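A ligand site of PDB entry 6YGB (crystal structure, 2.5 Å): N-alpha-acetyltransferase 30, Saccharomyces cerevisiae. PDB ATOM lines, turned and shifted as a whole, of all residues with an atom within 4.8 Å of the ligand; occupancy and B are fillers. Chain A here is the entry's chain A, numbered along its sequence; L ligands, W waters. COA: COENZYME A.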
ATOM      1  N   ASP A  26      27.079   0.668   0.222  1.00  0.00           N
ATOM      2  CA  ASP A  26      28.137   0.467  -0.751  1.00  0.00           C
ATOM      3  C   ASP A  26      29.529   0.348  -0.137  1.00  0.00           C
ATOM      4  O   ASP A  26      30.464  -0.074  -0.818  1.00  0.00           O
ATOM      5  CB  ASP A  26      28.146   1.610  -1.770  1.00  0.00           C
ATOM      6  CG  ASP A  26      26.831   1.746  -2.495  1.00  0.00           C
ATOM      7  OD1 ASP A  26      26.321   0.724  -3.015  1.00  0.00           O
ATOM      8  OD2 ASP A  26      26.292   2.874  -2.543  1.00  0.00           O
ATOM      9  N   ILE A  81      35.477  15.925  -1.491  1.00  0.00           N
ATOM     10  CA  ILE A  81      34.310  15.064  -1.673  1.00  0.00           C
ATOM     11  C   ILE A  81      34.583  13.778  -0.915  1.00  0.00           C
ATOM     12  O   ILE A  81      35.430  12.978  -1.317  1.00  0.00           O
ATOM     13  CB  ILE A  81      34.035  14.799  -3.158  1.00  0.00           C
ATOM     14  CG1 ILE A  81      33.823  16.120  -3.891  1.00  0.00           C
ATOM     15  CG2 ILE A  81      32.805  13.923  -3.329  1.00  0.00           C
ATOM     16  CD1 ILE A  81      33.588  15.963  -5.373  1.00  0.00           C
ATOM     17  N   LEU A  84      29.847   9.710  -1.878  1.00  0.00           N
ATOM     18  CA  LEU A  84      28.979   9.799  -3.050  1.00  0.00           C
ATOM     19  C   LEU A  84      28.273   8.454  -3.212  1.00  0.00           C
ATOM     20  O   LEU A  84      28.945   7.422  -3.330  1.00  0.00           O
ATOM     21  CB  LEU A  84      29.770  10.138  -4.305  1.00  0.00           C
ATOM     22  CG  LEU A  84      28.977  10.118  -5.623  1.00  0.00           C
ATOM     23  CD1 LEU A  84      27.853  11.146  -5.584  1.00  0.00           C
ATOM     24  CD2 LEU A  84      29.895  10.361  -6.814  1.00  0.00           C
ATOM     25  N   ALA A  85      26.944   8.467  -3.221  1.00  0.00           N
ATOM     26  CA  ALA A  85      26.192   7.236  -3.370  1.00  0.00           C
ATOM     27  C   ALA A  85      24.926   7.483  -4.178  1.00  0.00           C
ATOM     28  O   ALA A  85      24.259   8.498  -4.004  1.00  0.00           O
ATOM     29  CB  ALA A  85      25.836   6.631  -2.002  1.00  0.00           C
ATOM     30  N   VAL A  86      24.610   6.535  -5.059  1.00  0.00           N
ATOM     31  CA  VAL A  86      23.365   6.544  -5.817  1.00  0.00           C
ATOM     32  C   VAL A  86      22.739   5.172  -5.682  1.00  0.00           C
ATOM     33  O   VAL A  86      23.432   4.152  -5.802  1.00  0.00           O
ATOM     34  CB  VAL A  86      23.590   6.901  -7.304  1.00  0.00           C
ATOM     35  CG1 VAL A  86      22.374   6.542  -8.141  1.00  0.00           C
ATOM     36  CG2 VAL A  86      23.898   8.390  -7.449  1.00  0.00           C
ATOM     37  N   TYR A  90      18.630   3.363  -9.423  1.00  0.00           N
ATOM     38  CA  TYR A  90      18.696   4.637 -10.121  1.00  0.00           C
ATOM     39  C   TYR A  90      20.036   4.883 -10.801  1.00  0.00           C
ATOM     40  O   TYR A  90      20.276   6.002 -11.265  1.00  0.00           O
ATOM     41  CB  TYR A  90      18.368   5.789  -9.162  1.00  0.00           C
ATOM     42  CG  TYR A  90      16.908   5.836  -8.770  1.00  0.00           C
ATOM     43  CD1 TYR A  90      16.397   4.992  -7.798  1.00  0.00           C
ATOM     44  CD2 TYR A  90      16.040   6.742  -9.376  1.00  0.00           C
ATOM     45  CE1 TYR A  90      15.060   5.038  -7.440  1.00  0.00           C
ATOM     46  CE2 TYR A  90      14.710   6.794  -9.024  1.00  0.00           C
ATOM     47  CZ  TYR A  90      14.220   5.945  -8.052  1.00  0.00           C
ATOM     48  OH  TYR A  90      12.895   6.003  -7.707  1.00  0.00           O
ATOM     49  N   ARG A  91      20.898   3.886 -10.876  1.00  0.00           N
ATOM     50  CA  ARG A  91      22.190   4.049 -11.527  1.00  0.00           C
ATOM     51  C   ARG A  91      22.013   4.213 -13.039  1.00  0.00           C
ATOM     52  O   ARG A  91      21.050   3.711 -13.640  1.00  0.00           O
ATOM     53  CB  ARG A  91      23.095   2.861 -11.243  1.00  0.00           C
ATOM     54  CG  ARG A  91      23.185   2.465  -9.777  1.00  0.00           C
ATOM     55  CD  ARG A  91      24.417   3.062  -9.119  1.00  0.00           C
ATOM     56  NE  ARG A  91      24.510   2.678  -7.705  1.00  0.00           N
ATOM     57  CZ  ARG A  91      25.098   1.572  -7.263  1.00  0.00           C
ATOM     58  NH1 ARG A  91      25.665   0.733  -8.126  1.00  0.00           N
ATOM     59  NH2 ARG A  91      25.133   1.306  -5.960  1.00  0.00           N
ATOM     60  N   GLY A  92      22.955   4.916 -13.657  1.00  0.00           N
ATOM     61  CA  GLY A  92      22.982   5.071 -15.102  1.00  0.00           C
ATOM     62  C   GLY A  92      22.086   6.161 -15.666  1.00  0.00           C
ATOM     63  O   GLY A  92      21.898   6.203 -16.887  1.00  0.00           O
ATOM     64  N   HIS A  93      21.550   7.041 -14.818  1.00  0.00           N
ATOM     65  CA  HIS A  93      20.672   8.109 -15.270  1.00  0.00           C
ATOM     66  C   HIS A  93      21.281   9.491 -15.084  1.00  0.00           C
ATOM     67  O   HIS A  93      20.554  10.497 -15.123  1.00  0.00           O
ATOM     68  CB  HIS A  93      19.327   8.049 -14.540  1.00  0.00           C
ATOM     69  CG  HIS A  93      18.524   6.834 -14.886  1.00  0.00           C
ATOM     70  ND1 HIS A  93      17.999   6.623 -16.144  1.00  0.00           N
ATOM     71  CD2 HIS A  93      18.148   5.771 -14.135  1.00  0.00           C
ATOM     72  CE1 HIS A  93      17.345   5.477 -16.157  1.00  0.00           C
ATOM     73  NE2 HIS A  93      17.413   4.941 -14.954  1.00  0.00           N
ATOM     74  N   GLY A  94      22.591   9.574 -14.872  1.00  0.00           N
ATOM     75  CA  GLY A  94      23.225  10.872 -14.722  1.00  0.00           C
ATOM     76  C   GLY A  94      23.010  11.537 -13.379  1.00  0.00           C
ATOM     77  O   GLY A  94      23.259  12.737 -13.250  1.00  0.00           O
ATOM     78  N   ILE A  95      22.542  10.796 -12.387  1.00  0.00           N
ATOM     79  CA  ILE A  95      22.248  11.387 -11.085  1.00  0.00           C
ATOM     80  C   ILE A  95      23.530  11.751 -10.346  1.00  0.00           C
ATOM     81  O   ILE A  95      23.669  12.859  -9.813  1.00  0.00           O
ATOM     82  CB  ILE A  95      21.358  10.444 -10.244  1.00  0.00           C
ATOM     83  CG1 ILE A  95      20.052  10.167 -10.975  1.00  0.00           C
ATOM     84  CG2 ILE A  95      21.101  11.039  -8.870  1.00  0.00           C
ATOM     85  CD1 ILE A  95      19.223   9.093 -10.312  1.00  0.00           C
ATOM     86  N   ALA A  96      24.476  10.815 -10.287  1.00  0.00           N
ATOM     87  CA  ALA A  96      25.744  11.088  -9.627  1.00  0.00           C
ATOM     88  C   ALA A  96      26.472  12.250 -10.271  1.00  0.00           C
ATOM     89  O   ALA A  96      27.011  13.123  -9.579  1.00  0.00           O
ATOM     90  CB  ALA A  96      26.638   9.838  -9.639  1.00  0.00           C
ATOM     91  N   LYS A  97      26.490  12.294 -11.612  1.00  0.00           N
ATOM     92  CA  LYS A  97      27.130  13.404 -12.303  1.00  0.00           C
ATOM     93  C   LYS A  97      26.500  14.726 -11.897  1.00  0.00           C
ATOM     94  O   LYS A  97      27.213  15.708 -11.650  1.00  0.00           O
ATOM     95  CB  LYS A  97      27.019  13.212 -13.815  1.00  0.00           C
ATOM     96  CG  LYS A  97      27.509  14.411 -14.615  1.00  0.00           C
ATOM     97  CD  LYS A  97      27.575  14.099 -16.105  1.00  0.00           C
ATOM     98  CE  LYS A  97      28.112  15.285 -16.888  1.00  0.00           C
ATOM     99  NZ  LYS A  97      28.334  14.954 -18.332  1.00  0.00           N
ATOM    100  N   LEU A 117      39.629  14.443  -4.054  1.00  0.00           N
ATOM    101  CA  LEU A 117      38.967  13.219  -3.652  1.00  0.00           C
ATOM    102  C   LEU A 117      39.933  12.060  -3.842  1.00  0.00           C
ATOM    103  O   LEU A 117      40.914  12.164  -4.576  1.00  0.00           O
ATOM    104  CB  LEU A 117      37.670  12.983  -4.436  1.00  0.00           C
ATOM    105  CG  LEU A 117      37.788  12.725  -5.943  1.00  0.00           C
ATOM    106  CD1 LEU A 117      37.710  11.239  -6.238  1.00  0.00           C
ATOM    107  CD2 LEU A 117      36.709  13.483  -6.718  1.00  0.00           C
ATOM    108  N   GLU A 118      39.656  10.963  -3.146  1.00  0.00           N
ATOM    109  CA  GLU A 118      40.360   9.719  -3.363  1.00  0.00           C
ATOM    110  C   GLU A 118      39.366   8.694  -3.877  1.00  0.00           C
ATOM    111  O   GLU A 118      38.178   8.731  -3.537  1.00  0.00           O
ATOM    112  CB  GLU A 118      41.023   9.196  -2.087  1.00  0.00           C
ATOM    113  CG  GLU A 118      41.880  10.204  -1.370  1.00  0.00           C
ATOM    114  CD  GLU A 118      41.149  10.837  -0.207  1.00  0.00           C
ATOM    115  OE1 GLU A 118      40.022  10.396   0.081  1.00  0.00           O
ATOM    116  OE2 GLU A 118      41.702  11.757   0.425  1.00  0.00           O
ATOM    117  N   THR A 119      39.861   7.768  -4.689  1.00  0.00           N
ATOM    118  CA  THR A 119      39.015   6.701  -5.204  1.00  0.00           C
ATOM    119  C   THR A 119      39.885   5.516  -5.572  1.00  0.00           C
ATOM    120  O   THR A 119      41.108   5.633  -5.691  1.00  0.00           O
ATOM    121  CB  THR A 119      38.194   7.168  -6.414  1.00  0.00           C
ATOM    122  OG1 THR A 119      37.356   6.097  -6.858  1.00  0.00           O
ATOM    123  CG2 THR A 119      39.104   7.605  -7.534  1.00  0.00           C
ATOM    124  N   ASN A 123      38.003   1.561  -9.740  1.00  0.00           N
ATOM    125  CA  ASN A 123      36.672   2.161  -9.875  1.00  0.00           C
ATOM    126  C   ASN A 123      36.630   2.945 -11.172  1.00  0.00           C
ATOM    127  O   ASN A 123      36.762   4.172 -11.210  1.00  0.00           O
ATOM    128  CB  ASN A 123      36.360   3.049  -8.664  1.00  0.00           C
ATOM    129  CG  ASN A 123      34.887   3.369  -8.546  1.00  0.00           C
ATOM    130  OD1 ASN A 123      34.143   3.302  -9.515  1.00  0.00           O
ATOM    131  ND2 ASN A 123      34.461   3.725  -7.335  1.00  0.00           N
ATOM    132  N   SER A 124      36.430   2.214 -12.272  1.00  0.00           N
ATOM    133  CA  SER A 124      36.396   2.826 -13.604  1.00  0.00           C
ATOM    134  C   SER A 124      35.270   3.844 -13.707  1.00  0.00           C
ATOM    135  O   SER A 124      35.418   4.886 -14.344  1.00  0.00           O
ATOM    136  CB  SER A 124      36.236   1.742 -14.662  1.00  0.00           C
ATOM    137  OG  SER A 124      37.163   0.689 -14.478  1.00  0.00           O
ATOM    138  N   ALA A 125      34.117   3.533 -13.110  1.00  0.00           N
ATOM    139  CA  ALA A 125      32.968   4.431 -13.181  1.00  0.00           C
ATOM    140  C   ALA A 125      33.251   5.761 -12.507  1.00  0.00           C
ATOM    141  O   ALA A 125      32.868   6.815 -13.020  1.00  0.00           O
ATOM    142  CB  ALA A 125      31.754   3.759 -12.543  1.00  0.00           C
ATOM    143  N   ALA A 126      33.916   5.732 -11.354  1.00  0.00           N
ATOM    144  CA  ALA A 126      34.222   6.974 -10.658  1.00  0.00           C
ATOM    145  C   ALA A 126      35.297   7.767 -11.382  1.00  0.00           C
ATOM    146  O   ALA A 126      35.215   8.991 -11.475  1.00  0.00           O
ATOM    147  CB  ALA A 126      34.651   6.674  -9.216  1.00  0.00           C
ATOM    148  N   ASN A 128      35.904   7.765 -14.616  1.00  0.00           N
ATOM    149  CA  ASN A 128      35.313   8.353 -15.814  1.00  0.00           C
ATOM    150  C   ASN A 128      34.509   9.602 -15.488  1.00  0.00           C
ATOM    151  O   ASN A 128      34.611  10.618 -16.176  1.00  0.00           O
ATOM    152  CB  ASN A 128      34.429   7.327 -16.523  1.00  0.00           C
ATOM    153  CG  ASN A 128      35.144   6.633 -17.642  1.00  0.00           C
ATOM    154  OD1 ASN A 128      34.956   6.956 -18.805  1.00  0.00           O
ATOM    155  ND2 ASN A 128      35.987   5.669 -17.292  1.00  0.00           N
ATOM    156  N   LEU A 129      33.681   9.535 -14.447  1.00  0.00           N
ATOM    157  CA  LEU A 129      32.887  10.671 -14.034  1.00  0.00           C
ATOM    158  C   LEU A 129      33.767  11.880 -13.737  1.00  0.00           C
ATOM    159  O   LEU A 129      33.519  12.993 -14.219  1.00  0.00           O
ATOM    160  CB  LEU A 129      32.049  10.298 -12.806  1.00  0.00           C
ATOM    161  CG  LEU A 129      30.912  11.198 -12.321  1.00  0.00           C
ATOM    162  CD1 LEU A 129      30.046  10.430 -11.330  1.00  0.00           C
ATOM    163  CD2 LEU A 129      31.447  12.468 -11.664  1.00  0.00           C
ATOM    164  N   TYR A 130      34.824  11.681 -12.950  1.00  0.00           N
ATOM    165  CA  TYR A 130      35.622  12.802 -12.448  1.00  0.00           C
ATOM    166  C   TYR A 130      36.603  13.321 -13.493  1.00  0.00           C
ATOM    167  O   TYR A 130      36.692  14.533 -13.701  1.00  0.00           O
ATOM    168  CB  TYR A 130      36.359  12.377 -11.179  1.00  0.00           C
ATOM    169  CG  TYR A 130      35.449  12.220 -10.000  1.00  0.00           C
ATOM    170  CD1 TYR A 130      34.500  13.188  -9.706  1.00  0.00           C
ATOM    171  CD2 TYR A 130      35.518  11.101  -9.181  1.00  0.00           C
ATOM    172  CE1 TYR A 130      33.646  13.058  -8.630  1.00  0.00           C
ATOM    173  CE2 TYR A 130      34.667  10.962  -8.097  1.00  0.00           C
ATOM    174  CZ  TYR A 130      33.734  11.946  -7.821  1.00  0.00           C
ATOM    175  OH  TYR A 130      32.893  11.811  -6.756  1.00  0.00           O
HETATM  176  N1A COA L   1      31.439   2.612 -16.317  1.00  0.00           N
HETATM  177  C2A COA L   1      32.228   3.648 -16.707  1.00  0.00           C
HETATM  178  N3A COA L   1      31.860   4.933 -16.436  1.00  0.00           N
HETATM  179  C4A COA L   1      30.715   5.192 -15.787  1.00  0.00           C
HETATM  180  C5A COA L   1      29.931   4.178 -15.405  1.00  0.00           C
HETATM  181  C6A COA L   1      30.312   2.871 -15.685  1.00  0.00           C
HETATM  182  N6A COA L   1      29.870   1.463 -15.508  1.00  0.00           N
HETATM  183  N7A COA L   1      28.842   4.677 -14.781  1.00  0.00           N
HETATM  184  C8A COA L   1      28.951   6.019 -14.769  1.00  0.00           C
HETATM  185  N9A COA L   1      30.092   6.315 -15.392  1.00  0.00           N
HETATM  186  C1B COA L   1      30.771   7.398 -15.709  1.00  0.00           C
HETATM  187  C2B COA L   1      30.627   7.729 -17.203  1.00  0.00           C
HETATM  188  O2B COA L   1      31.639   8.718 -17.575  1.00  0.00           O
HETATM  189  C3B COA L   1      29.412   8.270 -17.250  1.00  0.00           C
HETATM  190  O3B COA L   1      29.216   8.966 -18.507  1.00  0.00           O
HETATM  191  P3B COA L   1      28.845   8.104 -19.854  1.00  0.00           P
HETATM  192  O7A COA L   1      27.337   8.082 -20.031  1.00  0.00           O
HETATM  193  O8A COA L   1      29.474   8.758 -21.054  1.00  0.00           O
HETATM  194  O9A COA L   1      29.344   6.683 -19.749  1.00  0.00           O
HETATM  195  C4B COA L   1      29.435   9.287 -15.970  1.00  0.00           C
HETATM  196  O4B COA L   1      30.097   8.659 -15.022  1.00  0.00           O
HETATM  197  C5B COA L   1      28.033   9.627 -15.487  1.00  0.00           C
HETATM  198  O5B COA L   1      27.532   8.533 -14.685  1.00  0.00           O
HETATM  199  P1A COA L   1      26.171   8.747 -13.669  1.00  0.00           P
HETATM  200  O1A COA L   1      24.941   8.160 -14.350  1.00  0.00           O
HETATM  201  O2A COA L   1      25.964  10.200 -13.390  1.00  0.00           O
HETATM  202  O3A COA L   1      26.432   7.963 -12.234  1.00  0.00           O
HETATM  203  P2A COA L   1      25.352   7.007 -11.402  1.00  0.00           P
HETATM  204  O4A COA L   1      24.254   7.855 -10.780  1.00  0.00           O
HETATM  205  O5A COA L   1      24.734   6.009 -12.347  1.00  0.00           O
HETATM  206  O6A COA L   1      26.229   6.226 -10.228  1.00  0.00           O
HETATM  207  CBP COA L   1      28.395   5.970  -9.051  1.00  0.00           C
HETATM  208  CCP COA L   1      27.615   6.246 -10.382  1.00  0.00           C
HETATM  209  CDP COA L   1      29.934   5.863  -9.390  1.00  0.00           C
HETATM  210  CEP COA L   1      28.179   7.134  -8.041  1.00  0.00           C
HETATM  211  CAP COA L   1      27.888   4.635  -8.424  1.00  0.00           C
HETATM  212  OAP COA L   1      28.581   3.584  -8.952  1.00  0.00           O
HETATM  213  C9P COA L   1      28.081   4.665  -6.901  1.00  0.00           C
HETATM  214  O9P COA L   1      27.123   4.746  -6.191  1.00  0.00           O
HETATM  215  N8P COA L   1      29.419   4.597  -6.324  1.00  0.00           N
HETATM  216  C7P COA L   1      29.584   4.624  -4.862  1.00  0.00           C
HETATM  217  C6P COA L   1      31.061   4.423  -4.474  1.00  0.00           C
HETATM  218  C5P COA L   1      31.942   5.365  -5.259  1.00  0.00           C
HETATM  219  O5P COA L   1      32.292   5.063  -6.343  1.00  0.00           O
HETATM  220  N4P COA L   1      32.384   6.646  -4.663  1.00  0.00           N
HETATM  221  C3P COA L   1      33.258   7.576  -5.449  1.00  0.00           C
HETATM  222  C2P COA L   1      34.485   8.034  -4.610  1.00  0.00           C
HETATM  223  S1P COA L   1      34.211   9.710  -3.893  1.00  0.00           S
HETATM  224  O   HOH W   1      26.475   4.399 -12.836  1.00  0.00           O
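The side-chain amide oxygen of Asn 123 sits at hydrogen-bond distance from the backbone NH of Ala 126, 3.1 Å away.
O of Val 86 lies within hydrogen-bond range of NE of Arg 91.
The side-chain amide nitrogen (ND2) of Asn 128 is in hydrogen-bond range of the backbone carbonyl oxygen (O) of Ser 124, at 3.1 Å.
NH2 of Arg 91 lies within salt-bridge range of OD1 of Asp 26, 3.2 Å away.
Merely in contact with the ligand: Leu 84 (3.3 Å), Ala 85 (3.9 Å), Arg 91 (3.3 Å), His 93 (3.6 Å), Ile 95 (3.6 Å), Glu 118 (3.9 Å), Ala 125 (3.4 Å), Asn 128 (3.3 Å) and Leu 129 (3.4 Å).
Hydrophobic or aromatic side chains within 4 Å of the ligand: Leu 84, Val 86, Ile 95, Ala 96, Ala 125 and Leu 129.
Within 4 Å of the ligand: Leu 84, Ala 85, Val 86, Arg 91, Gly 92, His 93, Gly 94, Ile 95, Ala 96, Lys 97, Glu 118, Asn 123, Ala 125, Asn 128, Leu 129 and Tyr 130.
The backbone NH (N) of Val 86 sits at hydrogen-bond distance from an oxygen (O9P) of the ligand (3.3 Å).
A sulfur (S1P) of the ligand sits close to the side-chain hydroxyl of Tyr 130 (3.8 Å).
N of Gly 92 sits at hydrogen-bond distance from O5A of the ligand, at 2.5 Å.
An oxygen (O4A) of the ligand is in hydrogen-bond range of the backbone NH (N) of Ala 96 (3.0 Å).
The backbone NH of Gly 94 sits at hydrogen-bond distance from an oxygen (O1A) of the ligand (2.8 Å).
The backbone NH (N) of Lys 97 sits at hydrogen-bond distance from an oxygen (O2A) of the ligand (2.8 Å).
ND2 of Asn 123 lies within hydrogen-bond range of O5P of the ligand (2.7 Å).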
